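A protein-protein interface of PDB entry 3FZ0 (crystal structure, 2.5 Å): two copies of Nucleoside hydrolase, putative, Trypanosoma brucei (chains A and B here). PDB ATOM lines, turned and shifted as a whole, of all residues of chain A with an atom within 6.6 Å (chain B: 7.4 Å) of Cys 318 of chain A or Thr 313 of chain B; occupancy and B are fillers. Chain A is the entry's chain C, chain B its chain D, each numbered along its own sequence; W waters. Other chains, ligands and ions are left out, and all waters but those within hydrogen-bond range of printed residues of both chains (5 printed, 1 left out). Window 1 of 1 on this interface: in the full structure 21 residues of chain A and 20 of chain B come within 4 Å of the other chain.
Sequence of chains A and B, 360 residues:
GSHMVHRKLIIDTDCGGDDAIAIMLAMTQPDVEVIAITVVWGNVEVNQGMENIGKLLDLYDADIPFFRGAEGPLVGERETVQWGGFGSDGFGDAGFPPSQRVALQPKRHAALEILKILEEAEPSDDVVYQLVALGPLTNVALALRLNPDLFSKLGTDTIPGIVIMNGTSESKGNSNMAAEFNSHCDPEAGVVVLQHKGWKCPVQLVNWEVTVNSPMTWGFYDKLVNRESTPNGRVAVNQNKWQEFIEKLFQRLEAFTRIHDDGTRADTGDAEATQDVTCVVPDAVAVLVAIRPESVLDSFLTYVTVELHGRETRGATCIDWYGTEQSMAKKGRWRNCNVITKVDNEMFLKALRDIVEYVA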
ATOM      1  N   THR A 168     -35.487  24.748   5.007  1.00  0.00           N
ATOM      2  CA  THR A 168     -36.522  24.069   4.242  1.00  0.00           C
ATOM      3  C   THR A 168     -36.082  22.630   3.998  1.00  0.00           C
ATOM      4  O   THR A 168     -34.900  22.310   4.172  1.00  0.00           O
ATOM      5  CB  THR A 168     -36.686  24.720   2.872  1.00  0.00           C
ATOM      6  OG1 THR A 168     -35.611  24.275   2.022  1.00  0.00           O
ATOM      7  CG2 THR A 168     -36.702  26.279   2.991  1.00  0.00           C
ATOM      8  N   LEU A 194     -24.358  23.685  12.153  1.00  0.00           N
ATOM      9  CA  LEU A 194     -24.421  22.420  11.465  1.00  0.00           C
ATOM     10  C   LEU A 194     -23.034  21.830  11.244  1.00  0.00           C
ATOM     11  O   LEU A 194     -22.893  20.614  11.139  1.00  0.00           O
ATOM     12  CB  LEU A 194     -25.193  22.587  10.146  1.00  0.00           C
ATOM     13  CG  LEU A 194     -26.700  22.895  10.253  1.00  0.00           C
ATOM     14  CD1 LEU A 194     -27.267  23.373   8.911  1.00  0.00           C
ATOM     15  CD2 LEU A 194     -27.501  21.646  10.745  1.00  0.00           C
ATOM     16  N   TYR A 303     -26.395  14.568   5.618  1.00  0.00           N
ATOM     17  CA  TYR A 303     -25.571  15.739   5.721  1.00  0.00           C
ATOM     18  C   TYR A 303     -26.332  16.956   5.181  1.00  0.00           C
ATOM     19  O   TYR A 303     -26.861  16.951   4.037  1.00  0.00           O
ATOM     20  CB  TYR A 303     -24.251  15.564   4.952  1.00  0.00           C
ATOM     21  CG  TYR A 303     -23.419  16.840   4.904  1.00  0.00           C
ATOM     22  CD1 TYR A 303     -22.681  17.230   6.017  1.00  0.00           C
ATOM     23  CD2 TYR A 303     -23.398  17.677   3.757  1.00  0.00           C
ATOM     24  CE1 TYR A 303     -21.924  18.402   6.015  1.00  0.00           C
ATOM     25  CE2 TYR A 303     -22.626  18.862   3.736  1.00  0.00           C
ATOM     26  CZ  TYR A 303     -21.898  19.206   4.868  1.00  0.00           C
ATOM     27  OH  TYR A 303     -21.132  20.332   4.931  1.00  0.00           O
ATOM     28  N   VAL A 304     -26.330  18.008   5.996  1.00  0.00           N
ATOM     29  CA  VAL A 304     -27.008  19.241   5.695  1.00  0.00           C
ATOM     30  C   VAL A 304     -26.092  20.407   5.966  1.00  0.00           C
ATOM     31  O   VAL A 304     -25.363  20.381   6.943  1.00  0.00           O
ATOM     32  CB  VAL A 304     -28.280  19.405   6.536  1.00  0.00           C
ATOM     33  CG1 VAL A 304     -28.934  20.764   6.294  1.00  0.00           C
ATOM     34  CG2 VAL A 304     -29.295  18.239   6.216  1.00  0.00           C
ATOM     35  N   THR A 305     -26.118  21.417   5.084  1.00  0.00           N
ATOM     36  CA  THR A 305     -25.430  22.673   5.317  1.00  0.00           C
ATOM     37  C   THR A 305     -26.244  23.839   4.763  1.00  0.00           C
ATOM     38  O   THR A 305     -27.322  23.609   4.185  1.00  0.00           O
ATOM     39  CB  THR A 305     -23.993  22.672   4.765  1.00  0.00           C
ATOM     40  OG1 THR A 305     -23.269  23.752   5.372  1.00  0.00           O
ATOM     41  CG2 THR A 305     -23.969  22.837   3.234  1.00  0.00           C
ATOM     42  N   VAL A 306     -25.758  25.073   4.957  1.00  0.00           N
ATOM     43  CA  VAL A 306     -26.461  26.277   4.479  1.00  0.00           C
ATOM     44  C   VAL A 306     -25.606  26.998   3.437  1.00  0.00           C
ATOM     45  O   VAL A 306     -24.406  27.171   3.621  1.00  0.00           O
ATOM     46  CB  VAL A 306     -26.811  27.237   5.666  1.00  0.00           C
ATOM     47  CG1 VAL A 306     -27.658  28.410   5.203  1.00  0.00           C
ATOM     48  CG2 VAL A 306     -27.569  26.474   6.765  1.00  0.00           C
ATOM     49  N   GLU A 307     -26.208  27.378   2.320  1.00  0.00           N
ATOM     50  CA  GLU A 307     -25.509  28.138   1.283  1.00  0.00           C
ATOM     51  C   GLU A 307     -25.163  29.547   1.786  1.00  0.00           C
ATOM     52  O   GLU A 307     -26.032  30.238   2.305  1.00  0.00           O
ATOM     53  CB  GLU A 307     -26.361  28.227   0.022  1.00  0.00           C
ATOM     54  CG  GLU A 307     -25.774  29.166  -1.066  1.00  0.00           C
ATOM     55  CD  GLU A 307     -24.455  28.667  -1.632  1.00  0.00           C
ATOM     56  OE1 GLU A 307     -24.382  27.492  -2.023  1.00  0.00           O
ATOM     57  OE2 GLU A 307     -23.493  29.441  -1.706  1.00  0.00           O
ATOM     58  N   HIS A 309     -23.148  31.769  -0.351  1.00  0.00           N
ATOM     59  CA  HIS A 309     -22.579  32.594  -1.437  1.00  0.00           C
ATOM     60  C   HIS A 309     -23.453  32.801  -2.680  1.00  0.00           C
ATOM     61  O   HIS A 309     -23.048  33.482  -3.612  1.00  0.00           O
ATOM     62  CB  HIS A 309     -21.162  32.083  -1.842  1.00  0.00           C
ATOM     63  CG  HIS A 309     -20.258  31.815  -0.667  1.00  0.00           C
ATOM     64  ND1 HIS A 309     -19.939  32.781   0.267  1.00  0.00           N
ATOM     65  CD2 HIS A 309     -19.638  30.684  -0.265  1.00  0.00           C
ATOM     66  CE1 HIS A 309     -19.150  32.257   1.186  1.00  0.00           C
ATOM     67  NE2 HIS A 309     -18.951  30.984   0.884  1.00  0.00           N
ATOM     68  N   GLY A 310     -24.648  32.220  -2.700  1.00  0.00           N
ATOM     69  CA  GLY A 310     -25.500  32.310  -3.896  1.00  0.00           C
ATOM     70  C   GLY A 310     -26.179  33.669  -3.925  1.00  0.00           C
ATOM     71  O   GLY A 310     -26.306  34.344  -2.886  1.00  0.00           O
ATOM     72  N   ARG A 311     -26.598  34.076  -5.115  1.00  0.00           N
ATOM     73  CA  ARG A 311     -27.305  35.338  -5.291  1.00  0.00           C
ATOM     74  C   ARG A 311     -28.779  35.139  -4.929  1.00  0.00           C
ATOM     75  O   ARG A 311     -29.321  35.935  -4.182  1.00  0.00           O
ATOM     76  CB  ARG A 311     -27.166  35.844  -6.737  1.00  0.00           C
ATOM     77  CG  ARG A 311     -27.792  37.188  -7.001  1.00  0.00           C
ATOM     78  CD  ARG A 311     -27.598  37.623  -8.436  1.00  0.00           C
ATOM     79  NE  ARG A 311     -26.273  38.197  -8.666  1.00  0.00           N
ATOM     80  CZ  ARG A 311     -25.920  38.875  -9.757  1.00  0.00           C
ATOM     81  NH1 ARG A 311     -26.788  39.075 -10.739  1.00  0.00           N
ATOM     82  NH2 ARG A 311     -24.695  39.364  -9.871  1.00  0.00           N
ATOM     83  N   THR A 313     -29.871  32.069  -3.817  1.00  0.00           N
ATOM     84  CA  THR A 313     -29.886  30.965  -2.860  1.00  0.00           C
ATOM     85  C   THR A 313     -29.135  31.198  -1.523  1.00  0.00           C
ATOM     86  O   THR A 313     -28.961  30.233  -0.751  1.00  0.00           O
ATOM     87  CB  THR A 313     -29.300  29.690  -3.499  1.00  0.00           C
ATOM     88  OG1 THR A 313     -28.032  30.003  -4.088  1.00  0.00           O
ATOM     89  CG2 THR A 313     -30.258  29.091  -4.583  1.00  0.00           C
ATOM     90  N   ARG A 314     -28.693  32.422  -1.223  1.00  0.00           N
ATOM     91  CA  ARG A 314     -28.133  32.678   0.090  1.00  0.00           C
ATOM     92  C   ARG A 314     -29.183  32.299   1.171  1.00  0.00           C
ATOM     93  O   ARG A 314     -30.357  32.674   1.097  1.00  0.00           O
ATOM     94  CB  ARG A 314     -27.626  34.113   0.229  1.00  0.00           C
ATOM     95  CG  ARG A 314     -27.517  34.612   1.647  1.00  0.00           C
ATOM     96  CD  ARG A 314     -26.633  35.871   1.791  1.00  0.00           C
ATOM     97  NE  ARG A 314     -25.359  35.446   2.334  1.00  0.00           N
ATOM     98  CZ  ARG A 314     -24.915  35.651   3.565  1.00  0.00           C
ATOM     99  NH1 ARG A 314     -25.604  36.360   4.450  1.00  0.00           N
ATOM    100  NH2 ARG A 314     -23.729  35.147   3.880  1.00  0.00           N
ATOM    101  N   GLY A 315     -28.743  31.506   2.148  1.00  0.00           N
ATOM    102  CA  GLY A 315     -29.625  30.969   3.168  1.00  0.00           C
ATOM    103  C   GLY A 315     -30.306  29.663   2.802  1.00  0.00           C
ATOM    104  O   GLY A 315     -30.984  29.099   3.635  1.00  0.00           O
ATOM    105  N   ALA A 316     -30.154  29.167   1.566  1.00  0.00           N
ATOM    106  CA  ALA A 316     -30.770  27.900   1.229  1.00  0.00           C
ATOM    107  C   ALA A 316     -30.260  26.783   2.140  1.00  0.00           C
ATOM    108  O   ALA A 316     -29.139  26.829   2.647  1.00  0.00           O
ATOM    109  CB  ALA A 316     -30.565  27.522  -0.259  1.00  0.00           C
ATOM    110  N   THR A 317     -31.120  25.791   2.350  1.00  0.00           N
ATOM    111  CA  THR A 317     -30.765  24.577   3.046  1.00  0.00           C
ATOM    112  C   THR A 317     -30.324  23.561   1.999  1.00  0.00           C
ATOM    113  O   THR A 317     -31.081  23.245   1.087  1.00  0.00           O
ATOM    114  CB  THR A 317     -31.979  24.057   3.853  1.00  0.00           C
ATOM    115  OG1 THR A 317     -32.481  25.113   4.675  1.00  0.00           O
ATOM    116  CG2 THR A 317     -31.592  22.875   4.766  1.00  0.00           C
ATOM    117  N   CYS A 318     -29.101  23.065   2.121  1.00  0.00           N
ATOM    118  CA  CYS A 318     -28.584  22.064   1.175  1.00  0.00           C
ATOM    119  C   CYS A 318     -28.575  20.747   1.890  1.00  0.00           C
ATOM    120  O   CYS A 318     -27.968  20.623   2.980  1.00  0.00           O
ATOM    121  CB  CYS A 318     -27.174  22.411   0.713  1.00  0.00           C
ATOM    122  SG  CYS A 318     -27.072  24.132   0.259  1.00  0.00           S
ATOM    123  N   ILE A 319     -29.280  19.781   1.312  1.00  0.00           N
ATOM    124  CA  ILE A 319     -29.480  18.488   1.939  1.00  0.00           C
ATOM    125  C   ILE A 319     -28.950  17.394   1.044  1.00  0.00           C
ATOM    126  O   ILE A 319     -29.307  17.341  -0.146  1.00  0.00           O
ATOM    127  CB  ILE A 319     -30.969  18.257   2.182  1.00  0.00           C
ATOM    128  CG1 ILE A 319     -31.494  19.320   3.180  1.00  0.00           C
ATOM    129  CG2 ILE A 319     -31.243  16.791   2.601  1.00  0.00           C
ATOM    130  CD1 ILE A 319     -32.988  19.381   3.222  1.00  0.00           C
ATOM    131  N   ASP A 320     -28.092  16.530   1.606  1.00  0.00           N
ATOM    132  CA  ASP A 320     -27.520  15.427   0.841  1.00  0.00           C
ATOM    133  C   ASP A 320     -28.468  14.213   0.758  1.00  0.00           C
ATOM    134  O   ASP A 320     -28.290  13.173   1.421  1.00  0.00           O
ATOM    135  CB  ASP A 320     -26.177  15.049   1.427  1.00  0.00           C
ATOM    136  CG  ASP A 320     -25.285  14.311   0.425  1.00  0.00           C
ATOM    137  OD1 ASP A 320     -25.740  13.976  -0.719  1.00  0.00           O
ATOM    138  OD2 ASP A 320     -24.121  14.043   0.802  1.00  0.00           O
ATOM    139  N   TRP A 321     -29.485  14.346  -0.082  1.00  0.00           N
ATOM    140  CA  TRP A 321     -30.460  13.287  -0.273  1.00  0.00           C
ATOM    141  C   TRP A 321     -29.870  11.921  -0.678  1.00  0.00           C
ATOM    142  O   TRP A 321     -30.262  10.890  -0.146  1.00  0.00           O
ATOM    143  CB  TRP A 321     -31.505  13.765  -1.266  1.00  0.00           C
ATOM    144  CG  TRP A 321     -32.321  14.926  -0.711  1.00  0.00           C
ATOM    145  CD1 TRP A 321     -32.207  16.246  -1.037  1.00  0.00           C
ATOM    146  CD2 TRP A 321     -33.359  14.842   0.282  1.00  0.00           C
ATOM    147  NE1 TRP A 321     -33.102  16.989  -0.318  1.00  0.00           N
ATOM    148  CE2 TRP A 321     -33.830  16.152   0.497  1.00  0.00           C
ATOM    149  CE3 TRP A 321     -33.934  13.779   1.007  1.00  0.00           C
ATOM    150  CZ2 TRP A 321     -34.841  16.443   1.423  1.00  0.00           C
ATOM    151  CZ3 TRP A 321     -34.948  14.065   1.922  1.00  0.00           C
ATOM    152  CH2 TRP A 321     -35.390  15.393   2.124  1.00  0.00           C
ATOM    153  N   SER B 171     -35.528  20.783  -4.898  1.00  0.00           N
ATOM    154  CA  SER B 171     -34.069  20.752  -4.785  1.00  0.00           C
ATOM    155  C   SER B 171     -33.480  19.488  -4.144  1.00  0.00           C
ATOM    156  O   SER B 171     -32.522  19.568  -3.399  1.00  0.00           O
ATOM    157  CB  SER B 171     -33.526  22.046  -4.150  1.00  0.00           C
ATOM    158  OG  SER B 171     -33.937  22.071  -2.806  1.00  0.00           O
ATOM    159  N   ASN B 176     -25.218  17.925  -7.594  1.00  0.00           N
ATOM    160  CA  ASN B 176     -24.760  18.336  -6.252  1.00  0.00           C
ATOM    161  C   ASN B 176     -25.978  18.245  -5.312  1.00  0.00           C
ATOM    162  O   ASN B 176     -26.997  17.677  -5.717  1.00  0.00           O
ATOM    163  CB  ASN B 176     -24.056  19.687  -6.270  1.00  0.00           C
ATOM    164  CG  ASN B 176     -24.977  20.829  -6.698  1.00  0.00           C
ATOM    165  OD1 ASN B 176     -26.187  20.820  -6.418  1.00  0.00           O
ATOM    166  ND2 ASN B 176     -24.410  21.813  -7.391  1.00  0.00           N
ATOM    167  N   MET B 177     -25.895  18.737  -4.088  1.00  0.00           N
ATOM    168  CA  MET B 177     -26.979  18.556  -3.138  1.00  0.00           C
ATOM    169  C   MET B 177     -28.281  19.186  -3.644  1.00  0.00           C
ATOM    170  O   MET B 177     -29.365  18.705  -3.296  1.00  0.00           O
ATOM    171  CB  MET B 177     -26.605  19.103  -1.748  1.00  0.00           C
ATOM    172  CG  MET B 177     -25.510  18.335  -1.050  1.00  0.00           C
ATOM    173  SD  MET B 177     -24.785  19.193   0.360  1.00  0.00           S
ATOM    174  CE  MET B 177     -25.901  18.746   1.614  1.00  0.00           C
ATOM    175  N   ALA B 178     -28.188  20.251  -4.447  1.00  0.00           N
ATOM    176  CA  ALA B 178     -29.371  21.043  -4.791  1.00  0.00           C
ATOM    177  C   ALA B 178     -29.790  20.941  -6.254  1.00  0.00           C
ATOM    178  O   ALA B 178     -30.969  21.108  -6.573  1.00  0.00           O
ATOM    179  CB  ALA B 178     -29.166  22.479  -4.428  1.00  0.00           C
ATOM    180  N   ALA B 179     -28.835  20.636  -7.130  1.00  0.00           N
ATOM    181  CA  ALA B 179     -29.032  20.795  -8.557  1.00  0.00           C
ATOM    182  C   ALA B 179     -29.145  19.475  -9.320  1.00  0.00           C
ATOM    183  O   ALA B 179     -28.438  18.504  -9.037  1.00  0.00           O
ATOM    184  CB  ALA B 179     -27.892  21.654  -9.158  1.00  0.00           C
ATOM    185  N   HIS B 184     -27.197  21.569 -13.672  1.00  0.00           N
ATOM    186  CA  HIS B 184     -25.870  21.785 -13.122  1.00  0.00           C
ATOM    187  C   HIS B 184     -24.840  21.829 -14.255  1.00  0.00           C
ATOM    188  O   HIS B 184     -23.890  22.593 -14.198  1.00  0.00           O
ATOM    189  CB  HIS B 184     -25.534  20.684 -12.107  1.00  0.00           C
ATOM    190  CG  HIS B 184     -24.280  20.938 -11.326  1.00  0.00           C
ATOM    191  ND1 HIS B 184     -23.581  19.929 -10.695  1.00  0.00           N
ATOM    192  CD2 HIS B 184     -23.590  22.080 -11.083  1.00  0.00           C
ATOM    193  CE1 HIS B 184     -22.529  20.441 -10.078  1.00  0.00           C
ATOM    194  NE2 HIS B 184     -22.512  21.739 -10.302  1.00  0.00           N
ATOM    195  N   PRO B 187     -25.719  25.975 -16.079  1.00  0.00           N
ATOM    196  CA  PRO B 187     -26.653  26.861 -15.405  1.00  0.00           C
ATOM    197  C   PRO B 187     -26.889  28.135 -16.223  1.00  0.00           C
ATOM    198  O   PRO B 187     -28.035  28.617 -16.311  1.00  0.00           O
ATOM    199  CB  PRO B 187     -25.939  27.170 -14.080  1.00  0.00           C
ATOM    200  CG  PRO B 187     -24.958  26.056 -13.905  1.00  0.00           C
ATOM    201  CD  PRO B 187     -24.476  25.829 -15.307  1.00  0.00           C
ATOM    202  N   VAL B 306     -32.441  29.890 -12.700  1.00  0.00           N
ATOM    203  CA  VAL B 306     -31.360  29.011 -12.243  1.00  0.00           C
ATOM    204  C   VAL B 306     -30.272  29.816 -11.497  1.00  0.00           C
ATOM    205  O   VAL B 306     -29.849  30.856 -11.980  1.00  0.00           O
ATOM    206  CB  VAL B 306     -30.768  28.191 -13.418  1.00  0.00           C
ATOM    207  CG1 VAL B 306     -29.785  27.161 -12.907  1.00  0.00           C
ATOM    208  CG2 VAL B 306     -31.859  27.509 -14.201  1.00  0.00           C
ATOM    209  N   GLU B 307     -29.838  29.346 -10.326  1.00  0.00           N
ATOM    210  CA  GLU B 307     -28.721  29.941  -9.599  1.00  0.00           C
ATOM    211  C   GLU B 307     -27.411  29.807 -10.365  1.00  0.00           C
ATOM    212  O   GLU B 307     -27.070  28.740 -10.836  1.00  0.00           O
ATOM    213  CB  GLU B 307     -28.577  29.290  -8.223  1.00  0.00           C
ATOM    214  CG  GLU B 307     -27.376  29.755  -7.402  1.00  0.00           C
ATOM    215  CD  GLU B 307     -27.402  31.267  -7.070  1.00  0.00           C
ATOM    216  OE1 GLU B 307     -28.412  31.733  -6.497  1.00  0.00           O
ATOM    217  OE2 GLU B 307     -26.413  31.986  -7.358  1.00  0.00           O
ATOM    218  N   LEU B 308     -26.657  30.880 -10.488  1.00  0.00           N
ATOM    219  CA  LEU B 308     -25.380  30.797 -11.198  1.00  0.00           C
ATOM    220  C   LEU B 308     -24.193  30.866 -10.256  1.00  0.00           C
ATOM    221  O   LEU B 308     -23.099  30.393 -10.631  1.00  0.00           O
ATOM    222  CB  LEU B 308     -25.237  31.922 -12.232  1.00  0.00           C
ATOM    223  CG  LEU B 308     -26.292  32.050 -13.319  1.00  0.00           C
ATOM    224  CD1 LEU B 308     -26.017  33.244 -14.148  1.00  0.00           C
ATOM    225  CD2 LEU B 308     -26.287  30.807 -14.151  1.00  0.00           C
ATOM    226  N   HIS B 309     -24.391  31.456  -9.062  1.00  0.00           N
ATOM    227  CA  HIS B 309     -23.256  31.935  -8.235  1.00  0.00           C
ATOM    228  C   HIS B 309     -23.035  31.237  -6.892  1.00  0.00           C
ATOM    229  O   HIS B 309     -22.069  31.540  -6.191  1.00  0.00           O
ATOM    230  CB  HIS B 309     -23.298  33.473  -8.046  1.00  0.00           C
ATOM    231  CG  HIS B 309     -23.542  34.235  -9.315  1.00  0.00           C
ATOM    232  ND1 HIS B 309     -22.750  34.093 -10.438  1.00  0.00           N
ATOM    233  CD2 HIS B 309     -24.522  35.104  -9.654  1.00  0.00           C
ATOM    234  CE1 HIS B 309     -23.224  34.851 -11.406  1.00  0.00           C
ATOM    235  NE2 HIS B 309     -24.297  35.475 -10.955  1.00  0.00           N
ATOM    236  N   GLY B 310     -23.903  30.322  -6.494  1.00  0.00           N
ATOM    237  CA  GLY B 310     -23.674  29.655  -5.216  1.00  0.00           C
ATOM    238  C   GLY B 310     -22.542  28.625  -5.271  1.00  0.00           C
ATOM    239  O   GLY B 310     -22.159  28.169  -6.334  1.00  0.00           O
ATOM    240  N   ARG B 311     -22.008  28.291  -4.108  1.00  0.00           N
ATOM    241  CA  ARG B 311     -20.984  27.269  -3.931  1.00  0.00           C
ATOM    242  C   ARG B 311     -21.668  25.892  -3.944  1.00  0.00           C
ATOM    243  O   ARG B 311     -21.383  25.063  -4.809  1.00  0.00           O
ATOM    244  CB  ARG B 311     -20.248  27.475  -2.589  1.00  0.00           C
ATOM    245  CG  ARG B 311     -19.095  26.527  -2.373  1.00  0.00           C
ATOM    246  CD  ARG B 311     -18.274  26.837  -1.145  1.00  0.00           C
ATOM    247  NE  ARG B 311     -17.390  27.978  -1.321  1.00  0.00           N
ATOM    248  CZ  ARG B 311     -16.471  28.352  -0.434  1.00  0.00           C
ATOM    249  NH1 ARG B 311     -16.330  27.667   0.687  1.00  0.00           N
ATOM    250  NH2 ARG B 311     -15.706  29.421  -0.655  1.00  0.00           N
ATOM    251  N   GLU B 312     -22.591  25.652  -3.010  1.00  0.00           N
ATOM    252  CA  GLU B 312     -23.317  24.383  -2.990  1.00  0.00           C
ATOM    253  C   GLU B 312     -24.542  24.378  -3.900  1.00  0.00           C
ATOM    254  O   GLU B 312     -25.052  23.317  -4.227  1.00  0.00           O
ATOM    255  CB  GLU B 312     -23.694  23.944  -1.564  1.00  0.00           C
ATOM    256  CG  GLU B 312     -22.525  23.693  -0.611  1.00  0.00           C
ATOM    257  CD  GLU B 312     -22.151  24.969   0.174  1.00  0.00           C
ATOM    258  OE1 GLU B 312     -22.679  26.068  -0.170  1.00  0.00           O
ATOM    259  OE2 GLU B 312     -21.329  24.895   1.132  1.00  0.00           O
ATOM    260  N   THR B 313     -25.000  25.538  -4.328  1.00  0.00           N
ATOM    261  CA  THR B 313     -26.253  25.658  -5.090  1.00  0.00           C
ATOM    262  C   THR B 313     -26.135  26.101  -6.558  1.00  0.00           C
ATOM    263  O   THR B 313     -27.144  26.413  -7.179  1.00  0.00           O
ATOM    264  CB  THR B 313     -27.205  26.644  -4.426  1.00  0.00           C
ATOM    265  OG1 THR B 313     -26.483  27.857  -4.141  1.00  0.00           O
ATOM    266  CG2 THR B 313     -27.777  26.050  -3.101  1.00  0.00           C
ATOM    267  N   ARG B 314     -24.931  26.120  -7.124  1.00  0.00           N
ATOM    268  CA  ARG B 314     -24.790  26.409  -8.535  1.00  0.00           C
ATOM    269  C   ARG B 314     -25.630  25.392  -9.308  1.00  0.00           C
ATOM    270  O   ARG B 314     -25.535  24.191  -9.052  1.00  0.00           O
ATOM    271  CB  ARG B 314     -23.300  26.406  -8.960  1.00  0.00           C
ATOM    272  CG  ARG B 314     -23.070  26.130 -10.436  1.00  0.00           C
ATOM    273  CD  ARG B 314     -21.720  26.614 -10.997  1.00  0.00           C
ATOM    274  NE  ARG B 314     -22.007  27.812 -11.734  1.00  0.00           N
ATOM    275  CZ  ARG B 314     -21.965  27.998 -13.043  1.00  0.00           C
ATOM    276  NH1 ARG B 314     -21.554  27.070 -13.900  1.00  0.00           N
ATOM    277  NH2 ARG B 314     -22.306  29.198 -13.476  1.00  0.00           N
ATOM    278  N   GLY B 315     -26.470  25.869 -10.234  1.00  0.00           N
ATOM    279  CA  GLY B 315     -27.366  24.968 -10.980  1.00  0.00           C
ATOM    280  C   GLY B 315     -28.716  24.689 -10.303  1.00  0.00           C
ATOM    281  O   GLY B 315     -29.571  24.061 -10.900  1.00  0.00           O
ATOM    282  N   ALA B 316     -28.923  25.156  -9.065  1.00  0.00           N
ATOM    283  CA  ALA B 316     -30.202  24.986  -8.403  1.00  0.00           C
ATOM    284  C   ALA B 316     -31.333  25.685  -9.165  1.00  0.00           C
ATOM    285  O   ALA B 316     -31.136  26.753  -9.771  1.00  0.00           O
ATOM    286  CB  ALA B 316     -30.152  25.486  -6.983  1.00  0.00           C
ATOM    287  N   THR B 317     -32.512  25.068  -9.123  1.00  0.00           N
ATOM    288  CA  THR B 317     -33.737  25.621  -9.660  1.00  0.00           C
ATOM    289  C   THR B 317     -34.387  26.412  -8.556  1.00  0.00           C
ATOM    290  O   THR B 317     -34.696  25.839  -7.519  1.00  0.00           O
ATOM    291  CB  THR B 317     -34.695  24.494 -10.072  1.00  0.00           C
ATOM    292  OG1 THR B 317     -33.985  23.572 -10.884  1.00  0.00           O
ATOM    293  CG2 THR B 317     -35.859  25.037 -10.818  1.00  0.00           C
ATOM    294  N   CYS B 318     -34.603  27.714  -8.804  1.00  0.00           N
ATOM    295  CA  CYS B 318     -35.211  28.626  -7.839  1.00  0.00           C
ATOM    296  C   CYS B 318     -36.598  28.894  -8.332  1.00  0.00           C
ATOM    297  O   CYS B 318     -36.785  29.292  -9.481  1.00  0.00           O
ATOM    298  CB  CYS B 318     -34.444  29.946  -7.755  1.00  0.00           C
ATOM    299  SG  CYS B 318     -32.684  29.727  -7.526  1.00  0.00           S
HETATM  300  O   HOH W   1     -17.107  30.290   2.584  1.00  0.00           O
HETATM  301  O   HOH W   2     -30.850  20.468  -1.180  1.00  0.00           O
HETATM  302  O   HOH W   3     -25.058  37.134 -12.842  1.00  0.00           O
HETATM  303  O   HOH W   4     -33.584  19.923  -0.739  1.00  0.00           O
HETATM  304  O   HOH W   5     -29.420  15.943  -3.051  1.00  0.00           O
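CE of Met 177 of chain B touches O of Tyr 303 of chain A, 3.2 Å away. CG2 of Thr 305 of chain A touches OE2 of Glu 312 of chain B, at 3.95 Å. CA of Gly 310 of chain A touches OE2 of Glu 307 of chain B, 3.6 Å away. Cys 318 of chain A touches Thr 313 of chain B (SG to CG2, 3.9 Å).
Of the printed residues of chain B, Arg 311 of chain A touches Glu 307 (3.1 Å) and His 309 (3.7 Å). Cys 318 of chain A touches just these residues of chain B: Met 177, Glu 312 and Thr 313. Of the printed residues of chain B, Asp 320 of chain A touches Met 177. Of the printed residues of chain A, Arg 311 of chain B touches Glu 307 and His 309. The nearest residue of chain B that does not touch Cys 318 of chain A is Ala 178 of chain B (5.4 Å).
The backbone carbonyl oxygen of Thr 305 of chain A lies within hydrogen-bond range of the backbone NH of Cys 318 of chain A (2.8 Å). The side-chain carboxylate of Glu 307 of chain B is in hydrogen-bond range of the backbone NH of Gly 310 of chain B (3.1 Å).
OE2 of Glu 307 of chain A is in hydrogen-bond range of N of Arg 311 of chain B (3.0 Å). The backbone NH (N) of Glu 312 of chain B is in hydrogen-bond range of the side-chain carboxylate (OE1) of Glu 307 of chain A (2.8 Å). The side-chain carboxylate (OE1) of Glu 307 of chain A lies within hydrogen-bond range of the side-chain hydroxyl (OG1) of Thr 313 of chain B. The side-chain carboxylate of Glu 307 of chain B is in hydrogen-bond range of the backbone NH of Arg 311 of chain A. OE1 of Glu 307 of chain B lies within hydrogen-bond range of OG1 of Thr 313 of chain A, 3.0 Å away. The side-chain hydroxyl of Thr 313 of chain A lies within hydrogen-bond range of the side-chain hydroxyl of Thr 313 of chain B (2.6 Å). O of His 309 of chain B sits close to O of His 309 of chain A (3.4 Å). The backbone carbonyl oxygen of Ile 319 of chain A sits close to the backbone carbonyl oxygen of Met 177 of chain B, at 3.4 Å.
Of the 19 printed residues of chain A, 10 touch a printed residue of chain B. Hydrophobic or aromatic side chains of chain A that line the printed part of chain B: Tyr 303 and His 309. Among the printed residues, 20 pairs touch across the chains. Among the printed residues, no Asp or Glu carboxylate lies within 4 Å of a Lys or Arg side-chain nitrogen of the other chain.
Water W4 bridges O of Ser 171 of chain B (2.9 Å) and NE1 of Trp 321 of chain A (3.0 Å).
Glu 307 of chain A touches Gly 310 of chain B, and with the chains exchanged Gly 310 of chain A touches Glu 307 of chain B. Glu 307 of chain A touches Arg 311 of chain B, and with the chains exchanged Arg 311 of chain A touches Glu 307 of chain B.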
